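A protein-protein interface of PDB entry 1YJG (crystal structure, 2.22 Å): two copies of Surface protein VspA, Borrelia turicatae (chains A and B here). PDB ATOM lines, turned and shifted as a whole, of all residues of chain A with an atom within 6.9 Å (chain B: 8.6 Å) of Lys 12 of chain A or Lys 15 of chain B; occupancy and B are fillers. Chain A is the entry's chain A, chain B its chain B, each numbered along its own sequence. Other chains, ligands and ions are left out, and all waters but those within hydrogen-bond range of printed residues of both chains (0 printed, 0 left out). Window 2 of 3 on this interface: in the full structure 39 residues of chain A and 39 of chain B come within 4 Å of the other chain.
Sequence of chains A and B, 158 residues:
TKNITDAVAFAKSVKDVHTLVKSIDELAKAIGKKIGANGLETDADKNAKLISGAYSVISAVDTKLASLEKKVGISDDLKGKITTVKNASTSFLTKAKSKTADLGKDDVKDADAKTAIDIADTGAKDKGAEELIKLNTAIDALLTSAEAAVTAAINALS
The side-chain amino group (NZ) of Lys 12 of chain B lies close to the side-chain amino group (NZ) of Lys 15 of chain A.
The side-chain carboxylate of Asp 16 of chain B is in hydrogen-bond range of the side-chain hydroxyl of Thr 19 of chain A (2.8 Å).
NZ of Lys 12 of chain A lies within salt-bridge range of OE2 of Glu 147 of chain B (3.96 Å).
The side-chain carboxylate of Asp 16 of chain A lies within hydrogen-bond range of the side-chain hydroxyl of Thr 19 of chain B (2.6 Å).
OD1 of Asp 16 of chain B lies within salt-bridge range of NZ of Lys 64 of chain B, at 2.6 Å.
The side-chain hydroxyl (OG1) of Thr 19 of chain A lies within hydrogen-bond range of the backbone carbonyl oxygen (O) of Lys 15 of chain A, 3.4 Å away.
O of Lys 15 of chain B lies within hydrogen-bond range of OG1 of Thr 19 of chain B (3.3 Å).
Lys 15 of chain B touches Lys 12 of chain A (CE to O, 3.7 Å).
Thr 19 of chain B touches Thr 19 of chain A.
Thr 19 of chain A touches Leu 20 of chain B.
Of chain B, only Lys 15 (3.7 Å) and Glu 147 (3.5 Å) come within 4 Å of Lys 12 of chain A.
No residue of chain B comes within 4 Å of Ala 11 of chain A.
Printed residues of chain B within 4 Å of Thr 19 of chain A: Asp 16, Thr 19 and Leu 20.
Of the printed residues of chain A, Thr 19 of chain B touches Asp 16 and Thr 19.
Of the printed residues of chain B, Lys 15 of chain A touches Lys 12.
Of the printed residues of chain A, Glu 147 of chain B touches Lys 12.
Of the printed residues of chain B, Asp 16 of chain A touches Thr 19.
The nearest residue of chain B that does not touch Lys 12 of chain A is Thr 19 of chain B (6.0 Å).
Of the 25 printed residues of chain B, 6 touch a printed residue of chain A.
Along chain B the printed residues that touch a printed residue of chain A span positions 12 to 147.
Printed residues of chain A that touch a printed residue of chain B: Lys 12, Lys 15, Asp 16 and Thr 19.
Among the printed residues, 7 pairs touch across the chains.
Lys 12 of chain A touches Lys 15 of chain B, and with the chains exchanged Lys 15 of chain A touches Lys 12 of chain B.
Asp 16 of chain A touches Thr 19 of chain B, and with the chains exchanged Thr 19 of chain A touches Asp 16 of chain B.
Thr 19 of chain A touches its own counterpart, Thr 19 of chain B.
Positions printed for both chains: 8, 9, 10, 11, 12, 13, 14, 15, 16, 17, 19, 143, 146 and 150.
Of the 7 pairs that touch across the chains among the printed residues, 5 have their exchanged pair printed and touching as well.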
ATOM      1  N   ALA A   7      34.324 -15.197  12.909  1.00  0.00           N
ATOM      2  CA  ALA A   7      33.239 -16.153  12.957  1.00  0.00           C
ATOM      3  C   ALA A   7      32.733 -16.392  11.553  1.00  0.00           C
ATOM      4  O   ALA A   7      32.499 -17.532  11.158  1.00  0.00           O
ATOM      5  CB  ALA A   7      32.106 -15.647  13.848  1.00  0.00           C
ATOM      6  N   VAL A   8      32.575 -15.309  10.803  1.00  0.00           N
ATOM      7  CA  VAL A   8      32.088 -15.397   9.435  1.00  0.00           C
ATOM      8  C   VAL A   8      33.080 -16.187   8.578  1.00  0.00           C
ATOM      9  O   VAL A   8      32.687 -17.103   7.864  1.00  0.00           O
ATOM     10  CB  VAL A   8      31.841 -13.997   8.849  1.00  0.00           C
ATOM     11  CG1 VAL A   8      31.648 -14.040   7.315  1.00  0.00           C
ATOM     12  CG2 VAL A   8      30.639 -13.351   9.527  1.00  0.00           C
ATOM     13  N   ALA A   9      34.362 -15.847   8.683  1.00  0.00           N
ATOM     14  CA  ALA A   9      35.407 -16.521   7.920  1.00  0.00           C
ATOM     15  C   ALA A   9      35.407 -18.034   8.193  1.00  0.00           C
ATOM     16  O   ALA A   9      35.455 -18.852   7.266  1.00  0.00           O
ATOM     17  CB  ALA A   9      36.777 -15.901   8.241  1.00  0.00           C
ATOM     18  N   PHE A  10      35.316 -18.399   9.466  1.00  0.00           N
ATOM     19  CA  PHE A  10      35.306 -19.800   9.872  1.00  0.00           C
ATOM     20  C   PHE A  10      34.088 -20.533   9.332  1.00  0.00           C
ATOM     21  O   PHE A  10      34.179 -21.667   8.876  1.00  0.00           O
ATOM     22  CB  PHE A  10      35.332 -19.909  11.399  1.00  0.00           C
ATOM     23  CG  PHE A  10      35.498 -21.307  11.891  1.00  0.00           C
ATOM     24  CD1 PHE A  10      36.757 -21.903  11.910  1.00  0.00           C
ATOM     25  CD2 PHE A  10      34.403 -22.038  12.315  1.00  0.00           C
ATOM     26  CE1 PHE A  10      36.907 -23.220  12.345  1.00  0.00           C
ATOM     27  CE2 PHE A  10      34.550 -23.352  12.760  1.00  0.00           C
ATOM     28  CZ  PHE A  10      35.788 -23.946  12.768  1.00  0.00           C
ATOM     29  N   ALA A  11      32.942 -19.870   9.402  1.00  0.00           N
ATOM     30  CA  ALA A  11      31.687 -20.423   8.922  1.00  0.00           C
ATOM     31  C   ALA A  11      31.749 -20.634   7.412  1.00  0.00           C
ATOM     32  O   ALA A  11      31.193 -21.599   6.903  1.00  0.00           O
ATOM     33  CB  ALA A  11      30.542 -19.500   9.272  1.00  0.00           C
ATOM     34  N   LYS A  12      32.419 -19.723   6.714  1.00  0.00           N
ATOM     35  CA  LYS A  12      32.568 -19.797   5.262  1.00  0.00           C
ATOM     36  C   LYS A  12      33.352 -21.045   4.885  1.00  0.00           C
ATOM     37  O   LYS A  12      33.039 -21.704   3.907  1.00  0.00           O
ATOM     38  CB  LYS A  12      33.361 -18.607   4.723  1.00  0.00           C
ATOM     39  CG  LYS A  12      32.561 -17.378   4.375  1.00  0.00           C
ATOM     40  CD  LYS A  12      33.492 -16.197   4.023  1.00  0.00           C
ATOM     41  CE  LYS A  12      34.358 -16.477   2.792  1.00  0.00           C
ATOM     42  NZ  LYS A  12      35.359 -15.394   2.510  1.00  0.00           N
ATOM     43  N   SER A  13      34.396 -21.322   5.661  1.00  0.00           N
ATOM     44  CA  SER A  13      35.269 -22.462   5.449  1.00  0.00           C
ATOM     45  C   SER A  13      34.563 -23.765   5.718  1.00  0.00           C
ATOM     46  O   SER A  13      34.762 -24.741   4.994  1.00  0.00           O
ATOM     47  CB  SER A  13      36.506 -22.359   6.345  1.00  0.00           C
ATOM     48  OG  SER A  13      37.377 -21.341   5.878  1.00  0.00           O
ATOM     49  N   VAL A  14      33.754 -23.786   6.772  1.00  0.00           N
ATOM     50  CA  VAL A  14      33.008 -24.973   7.147  1.00  0.00           C
ATOM     51  C   VAL A  14      31.891 -25.212   6.127  1.00  0.00           C
ATOM     52  O   VAL A  14      31.646 -26.353   5.728  1.00  0.00           O
ATOM     53  CB  VAL A  14      32.450 -24.860   8.582  1.00  0.00           C
ATOM     54  CG1 VAL A  14      31.533 -26.041   8.913  1.00  0.00           C
ATOM     55  CG2 VAL A  14      33.597 -24.801   9.586  1.00  0.00           C
ATOM     56  N   LYS A  15      31.228 -24.138   5.706  1.00  0.00           N
ATOM     57  CA  LYS A  15      30.144 -24.221   4.723  1.00  0.00           C
ATOM     58  C   LYS A  15      30.708 -24.850   3.455  1.00  0.00           C
ATOM     59  O   LYS A  15      30.094 -25.731   2.855  1.00  0.00           O
ATOM     60  CB  LYS A  15      29.566 -22.826   4.423  1.00  0.00           C
ATOM     61  CG  LYS A  15      28.370 -22.787   3.450  1.00  0.00           C
ATOM     62  CD  LYS A  15      27.266 -23.805   3.801  1.00  0.00           C
ATOM     63  CE  LYS A  15      26.111 -23.737   2.796  1.00  0.00           C
ATOM     64  NZ  LYS A  15      24.975 -24.595   3.174  1.00  0.00           N
ATOM     65  N   ASP A  16      31.895 -24.387   3.070  1.00  0.00           N
ATOM     66  CA  ASP A  16      32.589 -24.879   1.898  1.00  0.00           C
ATOM     67  C   ASP A  16      32.763 -26.407   1.975  1.00  0.00           C
ATOM     68  O   ASP A  16      32.390 -27.126   1.059  1.00  0.00           O
ATOM     69  CB  ASP A  16      33.938 -24.179   1.818  1.00  0.00           C
ATOM     70  CG  ASP A  16      34.725 -24.546   0.594  1.00  0.00           C
ATOM     71  OD1 ASP A  16      35.934 -24.835   0.763  1.00  0.00           O
ATOM     72  OD2 ASP A  16      34.237 -24.535  -0.567  1.00  0.00           O
ATOM     73  N   VAL A  17      33.319 -26.893   3.082  1.00  0.00           N
ATOM     74  CA  VAL A  17      33.537 -28.322   3.268  1.00  0.00           C
ATOM     75  C   VAL A  17      32.199 -29.099   3.298  1.00  0.00           C
ATOM     76  O   VAL A  17      32.091 -30.192   2.752  1.00  0.00           O
ATOM     77  CB  VAL A  17      34.366 -28.589   4.552  1.00  0.00           C
ATOM     78  CG1 VAL A  17      34.332 -30.062   4.938  1.00  0.00           C
ATOM     79  CG2 VAL A  17      35.789 -28.124   4.357  1.00  0.00           C
ATOM     80  N   THR A  19      29.367 -28.341   1.806  1.00  0.00           N
ATOM     81  CA  THR A  19      28.850 -28.439   0.446  1.00  0.00           C
ATOM     82  C   THR A  19      29.575 -29.550  -0.324  1.00  0.00           C
ATOM     83  O   THR A  19      28.923 -30.388  -0.949  1.00  0.00           O
ATOM     84  CB  THR A  19      28.989 -27.112  -0.273  1.00  0.00           C
ATOM     85  OG1 THR A  19      27.998 -26.194   0.231  1.00  0.00           O
ATOM     86  CG2 THR A  19      28.672 -27.262  -1.761  1.00  0.00           C
ATOM     87  N   LEU A 143      29.007 -27.594  11.113  1.00  0.00           N
ATOM     88  CA  LEU A 143      28.328 -26.471  10.456  1.00  0.00           C
ATOM     89  C   LEU A 143      27.373 -25.816  11.448  1.00  0.00           C
ATOM     90  O   LEU A 143      27.307 -24.588  11.538  1.00  0.00           O
ATOM     91  CB  LEU A 143      27.578 -26.885   9.171  1.00  0.00           C
ATOM     92  CG  LEU A 143      26.874 -25.748   8.394  1.00  0.00           C
ATOM     93  CD1 LEU A 143      27.847 -24.560   8.066  1.00  0.00           C
ATOM     94  CD2 LEU A 143      26.224 -26.238   7.118  1.00  0.00           C
ATOM     95  N   ALA A 146      29.408 -23.807  13.820  1.00  0.00           N
ATOM     96  CA  ALA A 146      29.985 -22.665  13.146  1.00  0.00           C
ATOM     97  C   ALA A 146      28.929 -21.594  12.884  1.00  0.00           C
ATOM     98  O   ALA A 146      29.209 -20.410  12.993  1.00  0.00           O
ATOM     99  CB  ALA A 146      30.617 -23.091  11.846  1.00  0.00           C
ATOM    100  N   VAL A 150      28.346 -17.561  14.416  1.00  0.00           N
ATOM    101  CA  VAL A 150      28.077 -16.394  13.586  1.00  0.00           C
ATOM    102  C   VAL A 150      26.888 -15.645  14.218  1.00  0.00           C
ATOM    103  O   VAL A 150      26.948 -14.439  14.418  1.00  0.00           O
ATOM    104  CB  VAL A 150      27.753 -16.779  12.104  1.00  0.00           C
ATOM    105  CG1 VAL A 150      27.251 -15.563  11.313  1.00  0.00           C
ATOM    106  CG2 VAL A 150      28.977 -17.368  11.417  1.00  0.00           C
ATOM    107  N   VAL B   8      22.836 -12.772   5.276  1.00  0.00           N
ATOM    108  CA  VAL B   8      23.675 -13.895   5.663  1.00  0.00           C
ATOM    109  C   VAL B   8      23.105 -15.118   4.964  1.00  0.00           C
ATOM    110  O   VAL B   8      23.846 -15.892   4.377  1.00  0.00           O
ATOM    111  CB  VAL B   8      23.695 -14.108   7.210  1.00  0.00           C
ATOM    112  CG1 VAL B   8      23.996 -15.573   7.584  1.00  0.00           C
ATOM    113  CG2 VAL B   8      24.710 -13.175   7.858  1.00  0.00           C
ATOM    114  N   ALA B   9      21.783 -15.261   5.023  1.00  0.00           N
ATOM    115  CA  ALA B   9      21.076 -16.376   4.407  1.00  0.00           C
ATOM    116  C   ALA B   9      21.263 -16.433   2.888  1.00  0.00           C
ATOM    117  O   ALA B   9      21.256 -17.517   2.311  1.00  0.00           O
ATOM    118  CB  ALA B   9      19.589 -16.310   4.751  1.00  0.00           C
ATOM    119  N   PHE B  10      21.429 -15.274   2.248  1.00  0.00           N
ATOM    120  CA  PHE B  10      21.621 -15.208   0.793  1.00  0.00           C
ATOM    121  C   PHE B  10      23.055 -15.594   0.440  1.00  0.00           C
ATOM    122  O   PHE B  10      23.276 -16.397  -0.461  1.00  0.00           O
ATOM    123  CB  PHE B  10      21.294 -13.816   0.234  1.00  0.00           C
ATOM    124  CG  PHE B  10      21.592 -13.668  -1.241  1.00  0.00           C
ATOM    125  CD1 PHE B  10      20.782 -14.272  -2.188  1.00  0.00           C
ATOM    126  CD2 PHE B  10      22.693 -12.934  -1.676  1.00  0.00           C
ATOM    127  CE1 PHE B  10      21.055 -14.139  -3.549  1.00  0.00           C
ATOM    128  CE2 PHE B  10      22.976 -12.804  -3.031  1.00  0.00           C
ATOM    129  CZ  PHE B  10      22.154 -13.403  -3.968  1.00  0.00           C
ATOM    130  N   ALA B  11      24.021 -15.011   1.151  1.00  0.00           N
ATOM    131  CA  ALA B  11      25.437 -15.301   0.927  1.00  0.00           C
ATOM    132  C   ALA B  11      25.749 -16.777   1.194  1.00  0.00           C
ATOM    133  O   ALA B  11      26.709 -17.302   0.659  1.00  0.00           O
ATOM    134  CB  ALA B  11      26.300 -14.421   1.791  1.00  0.00           C
ATOM    135  N   LYS B  12      24.936 -17.429   2.028  1.00  0.00           N
ATOM    136  CA  LYS B  12      25.094 -18.845   2.368  1.00  0.00           C
ATOM    137  C   LYS B  12      24.770 -19.658   1.113  1.00  0.00           C
ATOM    138  O   LYS B  12      25.508 -20.571   0.718  1.00  0.00           O
ATOM    139  CB  LYS B  12      24.110 -19.237   3.491  1.00  0.00           C
ATOM    140  CG  LYS B  12      24.709 -19.924   4.730  1.00  0.00           C
ATOM    141  CD  LYS B  12      23.692 -20.899   5.413  1.00  0.00           C
ATOM    142  CE  LYS B  12      23.958 -22.381   5.028  1.00  0.00           C
ATOM    143  NZ  LYS B  12      23.478 -23.435   5.987  1.00  0.00           N
ATOM    144  N   SER B  13      23.645 -19.303   0.494  1.00  0.00           N
ATOM    145  CA  SER B  13      23.160 -19.955  -0.716  1.00  0.00           C
ATOM    146  C   SER B  13      24.079 -19.737  -1.906  1.00  0.00           C
ATOM    147  O   SER B  13      24.274 -20.640  -2.720  1.00  0.00           O
ATOM    148  CB  SER B  13      21.741 -19.478  -1.028  1.00  0.00           C
ATOM    149  OG  SER B  13      20.849 -19.901  -0.008  1.00  0.00           O
ATOM    150  N   VAL B  14      24.658 -18.548  -2.010  1.00  0.00           N
ATOM    151  CA  VAL B  14      25.560 -18.257  -3.127  1.00  0.00           C
ATOM    152  C   VAL B  14      26.881 -19.016  -2.941  1.00  0.00           C
ATOM    153  O   VAL B  14      27.501 -19.443  -3.911  1.00  0.00           O
ATOM    154  CB  VAL B  14      25.818 -16.752  -3.276  1.00  0.00           C
ATOM    155  CG1 VAL B  14      26.814 -16.493  -4.390  1.00  0.00           C
ATOM    156  CG2 VAL B  14      24.517 -16.009  -3.561  1.00  0.00           C
ATOM    157  N   LYS B  15      27.292 -19.175  -1.688  1.00  0.00           N
ATOM    158  CA  LYS B  15      28.519 -19.878  -1.321  1.00  0.00           C
ATOM    159  C   LYS B  15      28.354 -21.376  -1.663  1.00  0.00           C
ATOM    160  O   LYS B  15      29.261 -22.018  -2.178  1.00  0.00           O
ATOM    161  CB  LYS B  15      28.780 -19.668   0.185  1.00  0.00           C
ATOM    162  CG  LYS B  15      30.146 -20.077   0.742  1.00  0.00           C
ATOM    163  CD  LYS B  15      31.267 -20.175  -0.274  1.00  0.00           C
ATOM    164  CE  LYS B  15      32.574 -20.568   0.399  1.00  0.00           C
ATOM    165  NZ  LYS B  15      33.748 -20.310  -0.482  1.00  0.00           N
ATOM    166  N   ASP B  16      27.169 -21.903  -1.405  1.00  0.00           N
ATOM    167  CA  ASP B  16      26.851 -23.298  -1.682  1.00  0.00           C
ATOM    168  C   ASP B  16      27.023 -23.563  -3.183  1.00  0.00           C
ATOM    169  O   ASP B  16      27.804 -24.417  -3.586  1.00  0.00           O
ATOM    170  CB  ASP B  16      25.427 -23.605  -1.205  1.00  0.00           C
ATOM    171  CG  ASP B  16      24.979 -25.027  -1.536  1.00  0.00           C
ATOM    172  OD1 ASP B  16      23.902 -25.176  -2.147  1.00  0.00           O
ATOM    173  OD2 ASP B  16      25.628 -26.043  -1.224  1.00  0.00           O
ATOM    174  N   VAL B  17      26.337 -22.787  -4.007  1.00  0.00           N
ATOM    175  CA  VAL B  17      26.427 -22.945  -5.450  1.00  0.00           C
ATOM    176  C   VAL B  17      27.867 -22.691  -5.937  1.00  0.00           C
ATOM    177  O   VAL B  17      28.337 -23.381  -6.836  1.00  0.00           O
ATOM    178  CB  VAL B  17      25.457 -21.984  -6.194  1.00  0.00           C
ATOM    179  CG1 VAL B  17      25.617 -22.131  -7.700  1.00  0.00           C
ATOM    180  CG2 VAL B  17      24.013 -22.240  -5.795  1.00  0.00           C
ATOM    181  N   HIS B  18      28.547 -21.705  -5.342  1.00  0.00           N
ATOM    182  CA  HIS B  18      29.927 -21.366  -5.706  1.00  0.00           C
ATOM    183  C   HIS B  18      30.879 -22.547  -5.504  1.00  0.00           C
ATOM    184  O   HIS B  18      31.644 -22.897  -6.394  1.00  0.00           O
ATOM    185  CB  HIS B  18      30.402 -20.157  -4.888  1.00  0.00           C
ATOM    186  CG  HIS B  18      31.761 -19.655  -5.266  1.00  0.00           C
ATOM    187  ND1 HIS B  18      32.923 -20.185  -4.743  1.00  0.00           N
ATOM    188  CD2 HIS B  18      32.143 -18.649  -6.089  1.00  0.00           C
ATOM    189  CE1 HIS B  18      33.961 -19.535  -5.241  1.00  0.00           C
ATOM    190  NE2 HIS B  18      33.515 -18.598  -6.062  1.00  0.00           N
ATOM    191  N   THR B  19      30.827 -23.155  -4.324  1.00  0.00           N
ATOM    192  CA  THR B  19      31.674 -24.301  -3.997  1.00  0.00           C
ATOM    193  C   THR B  19      31.385 -25.469  -4.949  1.00  0.00           C
ATOM    194  O   THR B  19      32.290 -26.196  -5.334  1.00  0.00           O
ATOM    195  CB  THR B  19      31.419 -24.727  -2.533  1.00  0.00           C
ATOM    196  OG1 THR B  19      32.048 -23.791  -1.648  1.00  0.00           O
ATOM    197  CG2 THR B  19      32.066 -26.091  -2.200  1.00  0.00           C
ATOM    198  N   LEU B  20      30.125 -25.635  -5.323  1.00  0.00           N
ATOM    199  CA  LEU B  20      29.733 -26.711  -6.228  1.00  0.00           C
ATOM    200  C   LEU B  20      30.395 -26.544  -7.614  1.00  0.00           C
ATOM    201  O   LEU B  20      30.847 -27.526  -8.224  1.00  0.00           O
ATOM    202  CB  LEU B  20      28.210 -26.777  -6.357  1.00  0.00           C
ATOM    203  CG  LEU B  20      27.421 -27.458  -5.232  1.00  0.00           C
ATOM    204  CD1 LEU B  20      25.953 -27.512  -5.626  1.00  0.00           C
ATOM    205  CD2 LEU B  20      27.911 -28.897  -4.897  1.00  0.00           C
ATOM    206  N   VAL B  21      30.485 -25.301  -8.081  1.00  0.00           N
ATOM    207  CA  VAL B  21      31.094 -25.006  -9.380  1.00  0.00           C
ATOM    208  C   VAL B  21      32.600 -25.256  -9.311  1.00  0.00           C
ATOM    209  O   VAL B  21      33.172 -25.839 -10.239  1.00  0.00           O
ATOM    210  CB  VAL B  21      30.774 -23.569  -9.856  1.00  0.00           C
ATOM    211  CG1 VAL B  21      31.596 -23.188 -11.086  1.00  0.00           C
ATOM    212  CG2 VAL B  21      29.290 -23.441 -10.150  1.00  0.00           C
ATOM    213  N   LYS B  22      33.229 -24.856  -8.208  1.00  0.00           N
ATOM    214  CA  LYS B  22      34.667 -25.064  -8.045  1.00  0.00           C
ATOM    215  C   LYS B  22      34.968 -26.543  -7.845  1.00  0.00           C
ATOM    216  O   LYS B  22      36.089 -26.993  -8.120  1.00  0.00           O
ATOM    217  CB  LYS B  22      35.243 -24.255  -6.874  1.00  0.00           C
ATOM    218  CG  LYS B  22      34.956 -22.766  -6.901  1.00  0.00           C
ATOM    219  CD  LYS B  22      35.412 -22.083  -8.186  1.00  0.00           C
ATOM    220  CE  LYS B  22      35.224 -20.567  -8.077  1.00  0.00           C
ATOM    221  NZ  LYS B  22      35.621 -19.818  -9.303  1.00  0.00           N
ATOM    222  N   VAL B  61      23.489 -27.132  -9.469  1.00  0.00           N
ATOM    223  CA  VAL B  61      23.803 -25.709  -9.448  1.00  0.00           C
ATOM    224  C   VAL B  61      22.693 -24.933 -10.160  1.00  0.00           C
ATOM    225  O   VAL B  61      22.253 -23.889  -9.684  1.00  0.00           O
ATOM    226  CB  VAL B  61      25.161 -25.435 -10.140  1.00  0.00           C
ATOM    227  CG1 VAL B  61      25.272 -23.986 -10.636  1.00  0.00           C
ATOM    228  CG2 VAL B  61      26.307 -25.775  -9.194  1.00  0.00           C
ATOM    229  N   LYS B  64      19.412 -24.978  -8.007  1.00  0.00           N
ATOM    230  CA  LYS B  64      19.546 -24.125  -6.827  1.00  0.00           C
ATOM    231  C   LYS B  64      19.460 -22.639  -7.203  1.00  0.00           C
ATOM    232  O   LYS B  64      18.959 -21.824  -6.428  1.00  0.00           O
ATOM    233  CB  LYS B  64      20.851 -24.422  -6.084  1.00  0.00           C
ATOM    234  CG  LYS B  64      20.834 -25.728  -5.303  1.00  0.00           C
ATOM    235  CD  LYS B  64      22.254 -26.198  -5.011  1.00  0.00           C
ATOM    236  CE  LYS B  64      22.280 -27.440  -4.149  1.00  0.00           C
ATOM    237  NZ  LYS B  64      22.204 -27.107  -2.701  1.00  0.00           N
ATOM    238  N   LEU B  68      16.800 -19.783  -6.192  1.00  0.00           N
ATOM    239  CA  LEU B  68      17.305 -18.503  -5.687  1.00  0.00           C
ATOM    240  C   LEU B  68      16.667 -17.293  -6.369  1.00  0.00           C
ATOM    241  O   LEU B  68      16.602 -16.218  -5.773  1.00  0.00           O
ATOM    242  CB  LEU B  68      18.820 -18.411  -5.860  1.00  0.00           C
ATOM    243  CG  LEU B  68      19.695 -18.466  -4.612  1.00  0.00           C
ATOM    244  CD1 LEU B  68      21.107 -18.074  -5.006  1.00  0.00           C
ATOM    245  CD2 LEU B  68      19.194 -17.565  -3.491  1.00  0.00           C
ATOM    246  N   ILE B 139      29.634 -16.807 -11.267  1.00  0.00           N
ATOM    247  CA  ILE B 139      29.379 -17.164  -9.869  1.00  0.00           C
ATOM    248  C   ILE B 139      30.293 -16.388  -8.927  1.00  0.00           C
ATOM    249  O   ILE B 139      29.904 -16.103  -7.799  1.00  0.00           O
ATOM    250  CB  ILE B 139      29.443 -18.717  -9.646  1.00  0.00           C
ATOM    251  CG1 ILE B 139      28.920 -19.103  -8.254  1.00  0.00           C
ATOM    252  CG2 ILE B 139      30.870 -19.260  -9.835  1.00  0.00           C
ATOM    253  CD1 ILE B 139      27.521 -18.584  -7.921  1.00  0.00           C
ATOM    254  N   LEU B 142      28.600 -13.002  -8.448  1.00  0.00           N
ATOM    255  CA  LEU B 142      27.446 -13.091  -7.562  1.00  0.00           C
ATOM    256  C   LEU B 142      27.869 -13.256  -6.093  1.00  0.00           C
ATOM    257  O   LEU B 142      27.231 -12.695  -5.201  1.00  0.00           O
ATOM    258  CB  LEU B 142      26.554 -14.252  -7.989  1.00  0.00           C
ATOM    259  CG  LEU B 142      25.239 -14.454  -7.230  1.00  0.00           C
ATOM    260  CD1 LEU B 142      24.251 -13.346  -7.540  1.00  0.00           C
ATOM    261  CD2 LEU B 142      24.645 -15.811  -7.570  1.00  0.00           C
ATOM    262  N   LEU B 143      28.937 -14.018  -5.840  1.00  0.00           N
ATOM    263  CA  LEU B 143      29.414 -14.233  -4.469  1.00  0.00           C
ATOM    264  C   LEU B 143      30.053 -12.960  -3.937  1.00  0.00           C
ATOM    265  O   LEU B 143      29.953 -12.657  -2.759  1.00  0.00           O
ATOM    266  CB  LEU B 143      30.417 -15.391  -4.393  1.00  0.00           C
ATOM    267  CG  LEU B 143      30.902 -15.841  -3.000  1.00  0.00           C
ATOM    268  CD1 LEU B 143      29.781 -16.481  -2.190  1.00  0.00           C
ATOM    269  CD2 LEU B 143      32.082 -16.819  -3.090  1.00  0.00           C
ATOM    270  N   THR B 144      30.705 -12.216  -4.814  1.00  0.00           N
ATOM    271  CA  THR B 144      31.355 -10.983  -4.414  1.00  0.00           C
ATOM    272  C   THR B 144      30.304  -9.967  -3.956  1.00  0.00           C
ATOM    273  O   THR B 144      30.480  -9.307  -2.934  1.00  0.00           O
ATOM    274  CB  THR B 144      32.217 -10.468  -5.569  1.00  0.00           C
ATOM    275  OG1 THR B 144      33.316 -11.371  -5.753  1.00  0.00           O
ATOM    276  CG2 THR B 144      32.881  -9.132  -5.239  1.00  0.00           C
ATOM    277  N   ALA B 146      27.240 -10.736  -2.943  1.00  0.00           N
ATOM    278  CA  ALA B 146      26.520 -11.283  -1.788  1.00  0.00           C
ATOM    279  C   ALA B 146      27.318 -11.084  -0.491  1.00  0.00           C
ATOM    280  O   ALA B 146      26.729 -10.866   0.576  1.00  0.00           O
ATOM    281  CB  ALA B 146      26.218 -12.761  -1.988  1.00  0.00           C
ATOM    282  N   GLU B 147      28.649 -11.158  -0.614  1.00  0.00           N
ATOM    283  CA  GLU B 147      29.585 -11.002   0.503  1.00  0.00           C
ATOM    284  C   GLU B 147      29.853  -9.522   0.814  1.00  0.00           C
ATOM    285  O   GLU B 147      30.370  -9.186   1.886  1.00  0.00           O
ATOM    286  CB  GLU B 147      30.888 -11.788   0.243  1.00  0.00           C
ATOM    287  CG  GLU B 147      30.703 -13.303   0.410  1.00  0.00           C
ATOM    288  CD  GLU B 147      31.976 -14.122   0.231  1.00  0.00           C
ATOM    289  OE1 GLU B 147      33.006 -13.561  -0.186  1.00  0.00           O
ATOM    290  OE2 GLU B 147      31.943 -15.342   0.510  1.00  0.00           O
ATOM    291  N   VAL B 150      26.788  -8.508   2.888  1.00  0.00           N
ATOM    292  CA  VAL B 150      26.963  -9.032   4.240  1.00  0.00           C
ATOM    293  C   VAL B 150      27.759  -8.003   5.053  1.00  0.00           C
ATOM    294  O   VAL B 150      27.434  -7.717   6.203  1.00  0.00           O
ATOM    295  CB  VAL B 150      27.706 -10.414   4.221  1.00  0.00           C
ATOM    296  CG1 VAL B 150      28.539 -10.639   5.484  1.00  0.00           C
ATOM    297  CG2 VAL B 150      26.714 -11.569   4.026  1.00  0.00           C
